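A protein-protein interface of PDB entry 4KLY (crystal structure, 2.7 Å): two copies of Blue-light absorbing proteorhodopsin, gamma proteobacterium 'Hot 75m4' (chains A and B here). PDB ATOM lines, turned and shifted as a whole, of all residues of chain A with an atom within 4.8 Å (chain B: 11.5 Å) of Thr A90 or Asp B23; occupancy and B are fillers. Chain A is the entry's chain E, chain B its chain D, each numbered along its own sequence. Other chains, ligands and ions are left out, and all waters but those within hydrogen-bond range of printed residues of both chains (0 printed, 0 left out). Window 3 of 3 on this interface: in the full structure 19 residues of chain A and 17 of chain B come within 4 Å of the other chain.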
ATOM      1  N   VAL A  83     -20.733 -25.372  21.361  1.00  0.00           N
ATOM      2  CA  VAL A  83     -19.976 -25.696  22.552  1.00  0.00           C
ATOM      3  C   VAL A  83     -20.100 -27.174  22.892  1.00  0.00           C
ATOM      4  O   VAL A  83     -19.117 -27.807  23.269  1.00  0.00           O
ATOM      5  CB  VAL A  83     -20.425 -24.842  23.748  1.00  0.00           C
ATOM      6  CG1 VAL A  83     -20.121 -25.540  25.070  1.00  0.00           C
ATOM      7  CG2 VAL A  83     -19.744 -23.484  23.698  1.00  0.00           C
ATOM      8  N   TRP A  84     -21.297 -27.732  22.740  1.00  0.00           N
ATOM      9  CA  TRP A  84     -21.523 -29.149  23.060  1.00  0.00           C
ATOM     10  C   TRP A  84     -20.815 -30.088  22.100  1.00  0.00           C
ATOM     11  O   TRP A  84     -20.643 -31.283  22.370  1.00  0.00           O
ATOM     12  CB  TRP A  84     -23.005 -29.460  23.013  1.00  0.00           C
ATOM     13  CG  TRP A  84     -23.326 -30.837  23.347  1.00  0.00           C
ATOM     14  CD1 TRP A  84     -23.713 -31.809  22.481  1.00  0.00           C
ATOM     15  CD2 TRP A  84     -23.306 -31.439  24.648  1.00  0.00           C
ATOM     16  NE1 TRP A  84     -23.968 -32.983  23.164  1.00  0.00           N
ATOM     17  CE2 TRP A  84     -23.719 -32.783  24.494  1.00  0.00           C
ATOM     18  CE3 TRP A  84     -22.983 -30.974  25.936  1.00  0.00           C
ATOM     19  CZ2 TRP A  84     -23.819 -33.664  25.569  1.00  0.00           C
ATOM     20  CZ3 TRP A  84     -23.087 -31.848  27.011  1.00  0.00           C
ATOM     21  CH2 TRP A  84     -23.498 -33.185  26.817  1.00  0.00           C
ATOM     22  N   GLY A  88     -17.996 -31.285  23.983  1.00  0.00           N
ATOM     23  CA  GLY A  88     -18.803 -32.108  24.873  1.00  0.00           C
ATOM     24  C   GLY A  88     -19.053 -31.544  26.267  1.00  0.00           C
ATOM     25  O   GLY A  88     -19.608 -32.252  27.101  1.00  0.00           O
ATOM     26  N   ASP A  89     -18.683 -30.283  26.527  1.00  0.00           N
ATOM     27  CA  ASP A  89     -18.940 -29.643  27.842  1.00  0.00           C
ATOM     28  C   ASP A  89     -20.295 -28.914  27.930  1.00  0.00           C
ATOM     29  O   ASP A  89     -20.746 -28.310  26.958  1.00  0.00           O
ATOM     30  CB  ASP A  89     -17.846 -28.633  28.166  1.00  0.00           C
ATOM     31  CG  ASP A  89     -16.478 -29.249  28.156  1.00  0.00           C
ATOM     32  OD1 ASP A  89     -16.315 -30.301  28.818  1.00  0.00           O
ATOM     33  OD2 ASP A  89     -15.574 -28.690  27.486  1.00  0.00           O
ATOM     34  N   THR A  90     -20.933 -28.961  29.098  1.00  0.00           N
ATOM     35  CA  THR A  90     -22.144 -28.166  29.333  1.00  0.00           C
ATOM     36  C   THR A  90     -21.829 -26.683  29.136  1.00  0.00           C
ATOM     37  O   THR A  90     -20.837 -26.191  29.668  1.00  0.00           O
ATOM     38  CB  THR A  90     -22.730 -28.397  30.738  1.00  0.00           C
ATOM     39  OG1 THR A  90     -23.426 -29.646  30.754  1.00  0.00           O
ATOM     40  CG2 THR A  90     -23.709 -27.293  31.134  1.00  0.00           C
ATOM     41  N   PRO A  91     -22.645 -25.980  28.331  1.00  0.00           N
ATOM     42  CA  PRO A  91     -22.425 -24.542  28.143  1.00  0.00           C
ATOM     43  C   PRO A  91     -23.173 -23.761  29.212  1.00  0.00           C
ATOM     44  O   PRO A  91     -24.179 -23.111  28.955  1.00  0.00           O
ATOM     45  CB  PRO A  91     -22.969 -24.284  26.735  1.00  0.00           C
ATOM     46  CG  PRO A  91     -24.017 -25.335  26.535  1.00  0.00           C
ATOM     47  CD  PRO A  91     -23.621 -26.532  27.368  1.00  0.00           C
ATOM     48  N   THR A  92     -22.659 -23.832  30.431  1.00  0.00           N
ATOM     49  CA  THR A  92     -23.300 -23.198  31.577  1.00  0.00           C
ATOM     50  C   THR A  92     -23.338 -21.706  31.443  1.00  0.00           C
ATOM     51  O   THR A  92     -24.344 -21.065  31.770  1.00  0.00           O
ATOM     52  CB  THR A  92     -22.573 -23.576  32.863  1.00  0.00           C
ATOM     53  OG1 THR A  92     -22.578 -25.005  32.947  1.00  0.00           O
ATOM     54  CG2 THR A  92     -23.260 -22.958  34.111  1.00  0.00           C
ATOM     55  N   VAL A  93     -22.240 -21.153  30.962  1.00  0.00           N
ATOM     56  CA  VAL A  93     -22.171 -19.719  30.852  1.00  0.00           C
ATOM     57  C   VAL A  93     -23.167 -19.234  29.807  1.00  0.00           C
ATOM     58  O   VAL A  93     -23.957 -18.359  30.111  1.00  0.00           O
ATOM     59  CB  VAL A  93     -20.750 -19.204  30.575  1.00  0.00           C
ATOM     60  CG1 VAL A  93     -20.716 -17.694  30.736  1.00  0.00           C
ATOM     61  CG2 VAL A  93     -19.760 -19.833  31.544  1.00  0.00           C
ATOM     62  N   PHE A  94     -23.186 -19.811  28.610  1.00  0.00           N
ATOM     63  CA  PHE A  94     -24.123 -19.307  27.602  1.00  0.00           C
ATOM     64  C   PHE A  94     -25.563 -19.487  28.082  1.00  0.00           C
ATOM     65  O   PHE A  94     -26.449 -18.659  27.801  1.00  0.00           O
ATOM     66  CB  PHE A  94     -23.959 -19.990  26.247  1.00  0.00           C
ATOM     67  CG  PHE A  94     -22.857 -19.430  25.406  1.00  0.00           C
ATOM     68  CD1 PHE A  94     -22.935 -18.141  24.901  1.00  0.00           C
ATOM     69  CD2 PHE A  94     -21.751 -20.213  25.065  1.00  0.00           C
ATOM     70  CE1 PHE A  94     -21.904 -17.637  24.110  1.00  0.00           C
ATOM     71  CE2 PHE A  94     -20.723 -19.707  24.287  1.00  0.00           C
ATOM     72  CZ  PHE A  94     -20.794 -18.418  23.813  1.00  0.00           C
ATOM     73  N   GLU A 143     -23.406 -24.497  39.424  1.00  0.00           N
ATOM     74  CA  GLU A 143     -22.975 -25.112  38.175  1.00  0.00           C
ATOM     75  C   GLU A 143     -21.568 -24.654  37.829  1.00  0.00           C
ATOM     76  O   GLU A 143     -20.717 -25.428  37.393  1.00  0.00           O
ATOM     77  CB  GLU A 143     -23.953 -24.755  37.041  1.00  0.00           C
ATOM     78  CG  GLU A 143     -25.420 -25.202  37.250  1.00  0.00           C
ATOM     79  CD  GLU A 143     -26.142 -25.646  35.966  1.00  0.00           C
ATOM     80  OE1 GLU A 143     -27.391 -25.619  35.936  1.00  0.00           O
ATOM     81  OE2 GLU A 143     -25.474 -26.033  34.973  1.00  0.00           O
ATOM     82  N   ALA A 218     -24.465 -34.864  32.913  1.00  0.00           N
ATOM     83  CA  ALA A 218     -24.530 -33.737  31.975  1.00  0.00           C
ATOM     84  C   ALA A 218     -25.482 -33.890  30.809  1.00  0.00           C
ATOM     85  O   ALA A 218     -25.812 -32.895  30.196  1.00  0.00           O
ATOM     86  CB  ALA A 218     -23.141 -33.437  31.426  1.00  0.00           C
ATOM     87  N   LEU A 221     -29.319 -33.311  32.273  1.00  0.00           N
ATOM     88  CA  LEU A 221     -29.314 -31.887  32.611  1.00  0.00           C
ATOM     89  C   LEU A 221     -29.692 -31.067  31.391  1.00  0.00           C
ATOM     90  O   LEU A 221     -30.717 -30.375  31.373  1.00  0.00           O
ATOM     91  CB  LEU A 221     -27.905 -31.496  33.108  1.00  0.00           C
ATOM     92  CG  LEU A 221     -27.502 -30.029  33.334  1.00  0.00           C
ATOM     93  CD1 LEU A 221     -28.328 -29.378  34.443  1.00  0.00           C
ATOM     94  CD2 LEU A 221     -26.014 -29.910  33.644  1.00  0.00           C
ATOM     95  N   ASN A 222     -28.862 -31.183  30.367  1.00  0.00           N
ATOM     96  CA  ASN A 222     -29.050 -30.431  29.148  1.00  0.00           C
ATOM     97  C   ASN A 222     -30.312 -30.798  28.366  1.00  0.00           C
ATOM     98  O   ASN A 222     -30.927 -29.905  27.770  1.00  0.00           O
ATOM     99  CB  ASN A 222     -27.807 -30.537  28.275  1.00  0.00           C
ATOM    100  CG  ASN A 222     -26.726 -29.582  28.720  1.00  0.00           C
ATOM    101  OD1 ASN A 222     -26.916 -28.354  28.697  1.00  0.00           O
ATOM    102  ND2 ASN A 222     -25.582 -30.120  29.116  1.00  0.00           N
ATOM    103  N   GLY B  21     -14.708 -21.537  19.974  1.00  0.00           N
ATOM    104  CA  GLY B  21     -15.427 -22.841  20.051  1.00  0.00           C
ATOM    105  C   GLY B  21     -15.828 -23.263  21.453  1.00  0.00           C
ATOM    106  O   GLY B  21     -16.641 -24.178  21.606  1.00  0.00           O
ATOM    107  N   GLY B  22     -15.262 -22.610  22.475  1.00  0.00           N
ATOM    108  CA  GLY B  22     -15.586 -22.914  23.879  1.00  0.00           C
ATOM    109  C   GLY B  22     -16.748 -22.099  24.432  1.00  0.00           C
ATOM    110  O   GLY B  22     -17.411 -21.353  23.697  1.00  0.00           O
ATOM    111  N   ASP B  23     -17.003 -22.258  25.734  1.00  0.00           N
ATOM    112  CA  ASP B  23     -18.028 -21.480  26.463  1.00  0.00           C
ATOM    113  C   ASP B  23     -17.447 -20.080  26.723  1.00  0.00           C
ATOM    114  O   ASP B  23     -16.271 -19.843  26.460  1.00  0.00           O
ATOM    115  CB  ASP B  23     -18.388 -22.199  27.779  1.00  0.00           C
ATOM    116  CG  ASP B  23     -19.739 -21.755  28.405  1.00  0.00           C
ATOM    117  OD1 ASP B  23     -20.493 -20.911  27.847  1.00  0.00           O
ATOM    118  OD2 ASP B  23     -20.039 -22.277  29.510  1.00  0.00           O
ATOM    119  N   LEU B  24     -18.267 -19.145  27.194  1.00  0.00           N
ATOM    120  CA  LEU B  24     -17.778 -17.807  27.535  1.00  0.00           C
ATOM    121  C   LEU B  24     -16.859 -17.884  28.759  1.00  0.00           C
ATOM    122  O   LEU B  24     -17.086 -18.677  29.694  1.00  0.00           O
ATOM    123  CB  LEU B  24     -18.941 -16.852  27.847  1.00  0.00           C
ATOM    124  CG  LEU B  24     -19.880 -16.344  26.746  1.00  0.00           C
ATOM    125  CD1 LEU B  24     -21.206 -15.899  27.354  1.00  0.00           C
ATOM    126  CD2 LEU B  24     -19.248 -15.210  25.965  1.00  0.00           C
ATOM    127  N   ASP B  25     -15.824 -17.055  28.749  1.00  0.00           N
ATOM    128  CA  ASP B  25     -14.955 -16.930  29.896  1.00  0.00           C
ATOM    129  C   ASP B  25     -15.705 -16.127  30.953  1.00  0.00           C
ATOM    130  O   ASP B  25     -15.927 -14.924  30.777  1.00  0.00           O
ATOM    131  CB  ASP B  25     -13.654 -16.227  29.505  1.00  0.00           C
ATOM    132  CG  ASP B  25     -12.455 -16.829  30.169  1.00  0.00           C
ATOM    133  OD1 ASP B  25     -12.613 -17.315  31.319  1.00  0.00           O
ATOM    134  OD2 ASP B  25     -11.372 -16.823  29.530  1.00  0.00           O
ATOM    135  N   ILE B  26     -16.122 -16.804  32.028  1.00  0.00           N
ATOM    136  CA  ILE B  26     -16.801 -16.147  33.162  1.00  0.00           C
ATOM    137  C   ILE B  26     -15.822 -15.304  33.979  1.00  0.00           C
ATOM    138  O   ILE B  26     -16.206 -14.298  34.582  1.00  0.00           O
ATOM    139  CB  ILE B  26     -17.554 -17.153  34.072  1.00  0.00           C
ATOM    140  CG1 ILE B  26     -18.245 -16.427  35.241  1.00  0.00           C
ATOM    141  CG2 ILE B  26     -16.638 -18.258  34.583  1.00  0.00           C
ATOM    142  CD1 ILE B  26     -19.197 -15.311  34.827  1.00  0.00           C
ATOM    143  N   SER B  27     -14.557 -15.711  33.973  1.00  0.00           N
ATOM    144  CA  SER B  27     -13.489 -14.908  34.549  1.00  0.00           C
ATOM    145  C   SER B  27     -13.343 -13.557  33.840  1.00  0.00           C
ATOM    146  O   SER B  27     -12.900 -12.594  34.464  1.00  0.00           O
ATOM    147  CB  SER B  27     -12.171 -15.672  34.516  1.00  0.00           C
ATOM    148  OG  SER B  27     -11.883 -16.114  33.204  1.00  0.00           O
ATOM    149  N   ASP B  28     -13.720 -13.482  32.555  1.00  0.00           N
ATOM    150  CA  ASP B  28     -13.704 -12.220  31.788  1.00  0.00           C
ATOM    151  C   ASP B  28     -15.019 -11.431  31.983  1.00  0.00           C
ATOM    152  O   ASP B  28     -15.936 -11.474  31.167  1.00  0.00           O
ATOM    153  CB  ASP B  28     -13.418 -12.495  30.305  1.00  0.00           C
ATOM    154  CG  ASP B  28     -12.998 -11.238  29.540  1.00  0.00           C
ATOM    155  OD1 ASP B  28     -12.965 -10.158  30.164  1.00  0.00           O
ATOM    156  OD2 ASP B  28     -12.700 -11.307  28.319  1.00  0.00           O
ATOM    157  N   THR B  29     -15.088 -10.708  33.091  1.00  0.00           N
ATOM    158  CA  THR B  29     -16.248  -9.895  33.446  1.00  0.00           C
ATOM    159  C   THR B  29     -16.533  -8.835  32.386  1.00  0.00           C
ATOM    160  O   THR B  29     -17.688  -8.416  32.216  1.00  0.00           O
ATOM    161  CB  THR B  29     -16.027  -9.221  34.832  1.00  0.00           C
ATOM    162  OG1 THR B  29     -15.844 -10.241  35.813  1.00  0.00           O
ATOM    163  CG2 THR B  29     -17.209  -8.336  35.252  1.00  0.00           C
ATOM    164  N   GLY B  31     -15.694  -9.118  29.005  1.00  0.00           N
ATOM    165  CA  GLY B  31     -16.253  -9.865  27.874  1.00  0.00           C
ATOM    166  C   GLY B  31     -17.715 -10.258  28.075  1.00  0.00           C
ATOM    167  O   GLY B  31     -18.477 -10.365  27.122  1.00  0.00           O
ATOM    168  N   VAL B  32     -18.122 -10.461  29.314  1.00  0.00           N
ATOM    169  CA  VAL B  32     -19.485 -10.852  29.573  1.00  0.00           C
ATOM    170  C   VAL B  32     -20.464  -9.669  29.422  1.00  0.00           C
ATOM    171  O   VAL B  32     -21.521  -9.834  28.838  1.00  0.00           O
ATOM    172  CB  VAL B  32     -19.613 -11.562  30.950  1.00  0.00           C
ATOM    173  CG1 VAL B  32     -21.075 -11.854  31.284  1.00  0.00           C
ATOM    174  CG2 VAL B  32     -18.790 -12.853  30.952  1.00  0.00           C
ATOM    175  N   TRP B  35     -20.877  -8.844  25.885  1.00  0.00           N
ATOM    176  CA  TRP B  35     -21.829  -9.765  25.334  1.00  0.00           C
ATOM    177  C   TRP B  35     -23.283  -9.306  25.635  1.00  0.00           C
ATOM    178  O   TRP B  35     -24.123  -9.156  24.734  1.00  0.00           O
ATOM    179  CB  TRP B  35     -21.577 -11.136  25.929  1.00  0.00           C
ATOM    180  CG  TRP B  35     -22.502 -12.122  25.347  1.00  0.00           C
ATOM    181  CD1 TRP B  35     -23.794 -12.301  25.682  1.00  0.00           C
ATOM    182  CD2 TRP B  35     -22.231 -13.026  24.270  1.00  0.00           C
ATOM    183  NE1 TRP B  35     -24.350 -13.245  24.885  1.00  0.00           N
ATOM    184  CE2 TRP B  35     -23.415 -13.710  24.007  1.00  0.00           C
ATOM    185  CE3 TRP B  35     -21.090 -13.316  23.496  1.00  0.00           C
ATOM    186  CZ2 TRP B  35     -23.514 -14.662  23.010  1.00  0.00           C
ATOM    187  CZ3 TRP B  35     -21.184 -14.271  22.506  1.00  0.00           C
ATOM    188  CH2 TRP B  35     -22.384 -14.925  22.263  1.00  0.00           C
ATOM    189  N   ARG B  81     -16.350  -5.884  21.337  1.00  0.00           N
ATOM    190  CA  ARG B  81     -16.150  -7.153  22.031  1.00  0.00           C
ATOM    191  C   ARG B  81     -15.055  -8.024  21.416  1.00  0.00           C
ATOM    192  O   ARG B  81     -14.310  -8.673  22.143  1.00  0.00           O
ATOM    193  CB  ARG B  81     -17.433  -7.962  22.105  1.00  0.00           C
ATOM    194  CG  ARG B  81     -17.197  -9.293  22.792  1.00  0.00           C
ATOM    195  CD  ARG B  81     -18.439  -9.874  23.428  1.00  0.00           C
ATOM    196  NE  ARG B  81     -18.054 -10.891  24.401  1.00  0.00           N
ATOM    197  CZ  ARG B  81     -17.653 -12.123  24.097  1.00  0.00           C
ATOM    198  NH1 ARG B  81     -17.594 -12.540  22.836  1.00  0.00           N
ATOM    199  NH2 ARG B  81     -17.312 -12.951  25.073  1.00  0.00           N
ATOM    200  N   ILE B  85     -11.556  -9.569  23.217  1.00  0.00           N
ATOM    201  CA  ILE B  85     -11.268 -11.006  23.177  1.00  0.00           C
ATOM    202  C   ILE B  85      -9.955 -11.381  22.476  1.00  0.00           C
ATOM    203  O   ILE B  85      -9.366 -12.414  22.773  1.00  0.00           O
ATOM    204  CB  ILE B  85     -12.481 -11.744  22.538  1.00  0.00           C
ATOM    205  CG1 ILE B  85     -13.391 -12.287  23.632  1.00  0.00           C
ATOM    206  CG2 ILE B  85     -12.076 -12.891  21.620  1.00  0.00           C
ATOM    207  CD1 ILE B  85     -13.814 -11.239  24.639  1.00  0.00           C
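Among the printed residues, merely in contact across the chains: Val A83 with Gly B22 (3.2 Å), Phe A94 with Trp B35 (3.3 Å), Val A93 with Leu B24 (3.5 Å), Pro A91 with Asp B23 (3.5 Å), Phe A94 with Leu B24 (3.6 Å), Val A83 with Asp B23 (3.6 Å), Phe A94 with Gly B22 (3.7 Å), Val A83 with Gly B21 (3.8 Å) and Thr A90 with Asp B23 (3.998 Å).
N of Phe A94 sits at hydrogen-bond distance from OD1 of Asp B23.
OD2 of Asp B23 sits at hydrogen-bond distance from N of Thr A92 (3.2 Å).
The backbone NH of Val A93 lies within hydrogen-bond range of the side-chain carboxylate of Asp B23 (2.9 Å).
Printed residues of chain B that touch a printed residue of chain A: Gly B21, Gly B22, Asp B23, Leu B24 and Trp B35.
Hydrophobic or aromatic side chains of chain B within 4 Å of the printed part of chain A: Leu B24 and Trp B35.
Of the 13 printed residues of chain A, 6 touch a printed residue of chain B.
Hydrophobic or aromatic side chains of chain A within 4 Å of the printed part of chain B: Val A83, Val A93 and Phe A94.
Along chain A the printed residues that touch a printed residue of chain B span positions 83 to 94.
Printed residues of chain B within 4 Å of Val A83: Gly B21 (3.8 Å), Gly B22 (3.2 Å) and Asp B23 (3.6 Å).
No residue of chain B comes within 4 Å of Gly A88.
No residue of chain B comes within 4 Å of Asp A89.
Printed residues of chain B within 4 Å of Thr A90: Asp B23 (3.998 Å).
Thr A92 touches one residue of chain B.
Printed residues of chain B within 4 Å of Val A93: Asp B23 and Leu B24.
Printed residues of chain B within 4 Å of Phe A94: Gly B22 (3.7 Å), Asp B23 (3.0 Å), Leu B24 (3.6 Å) and Trp B35 (3.3 Å).
No residue of chain B comes within 4 Å of Ala A218.
Leu A221 touches none of the printed residues of chain B.
Of the printed residues of chain A, Gly B22 touches Val A83 (3.2 Å) and Phe A94 (3.7 Å).
Of the printed residues of chain A, Asp B23 touches Val A83, Thr A90, Pro A91, Thr A92, Val A93 and Phe A94.
Of the printed residues of chain A, Leu B24 touches Val A93 (3.5 Å) and Phe A94 (3.6 Å).
Ser B27 touches none of the printed residues of chain A.
The nearest printed residue of chain A that does not touch Asp B23 is Asp A89 (6.5 Å).
No position is printed for both chains.
Of the 12 pairs that touch across the chains among the printed residues, none has its exchanged pair printed and touching as well.
The side-chain hydroxyl (OG1) of Thr A90 is in hydrogen-bond range of the side-chain amide nitrogen (ND2) of Asn A222 (2.7 Å).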
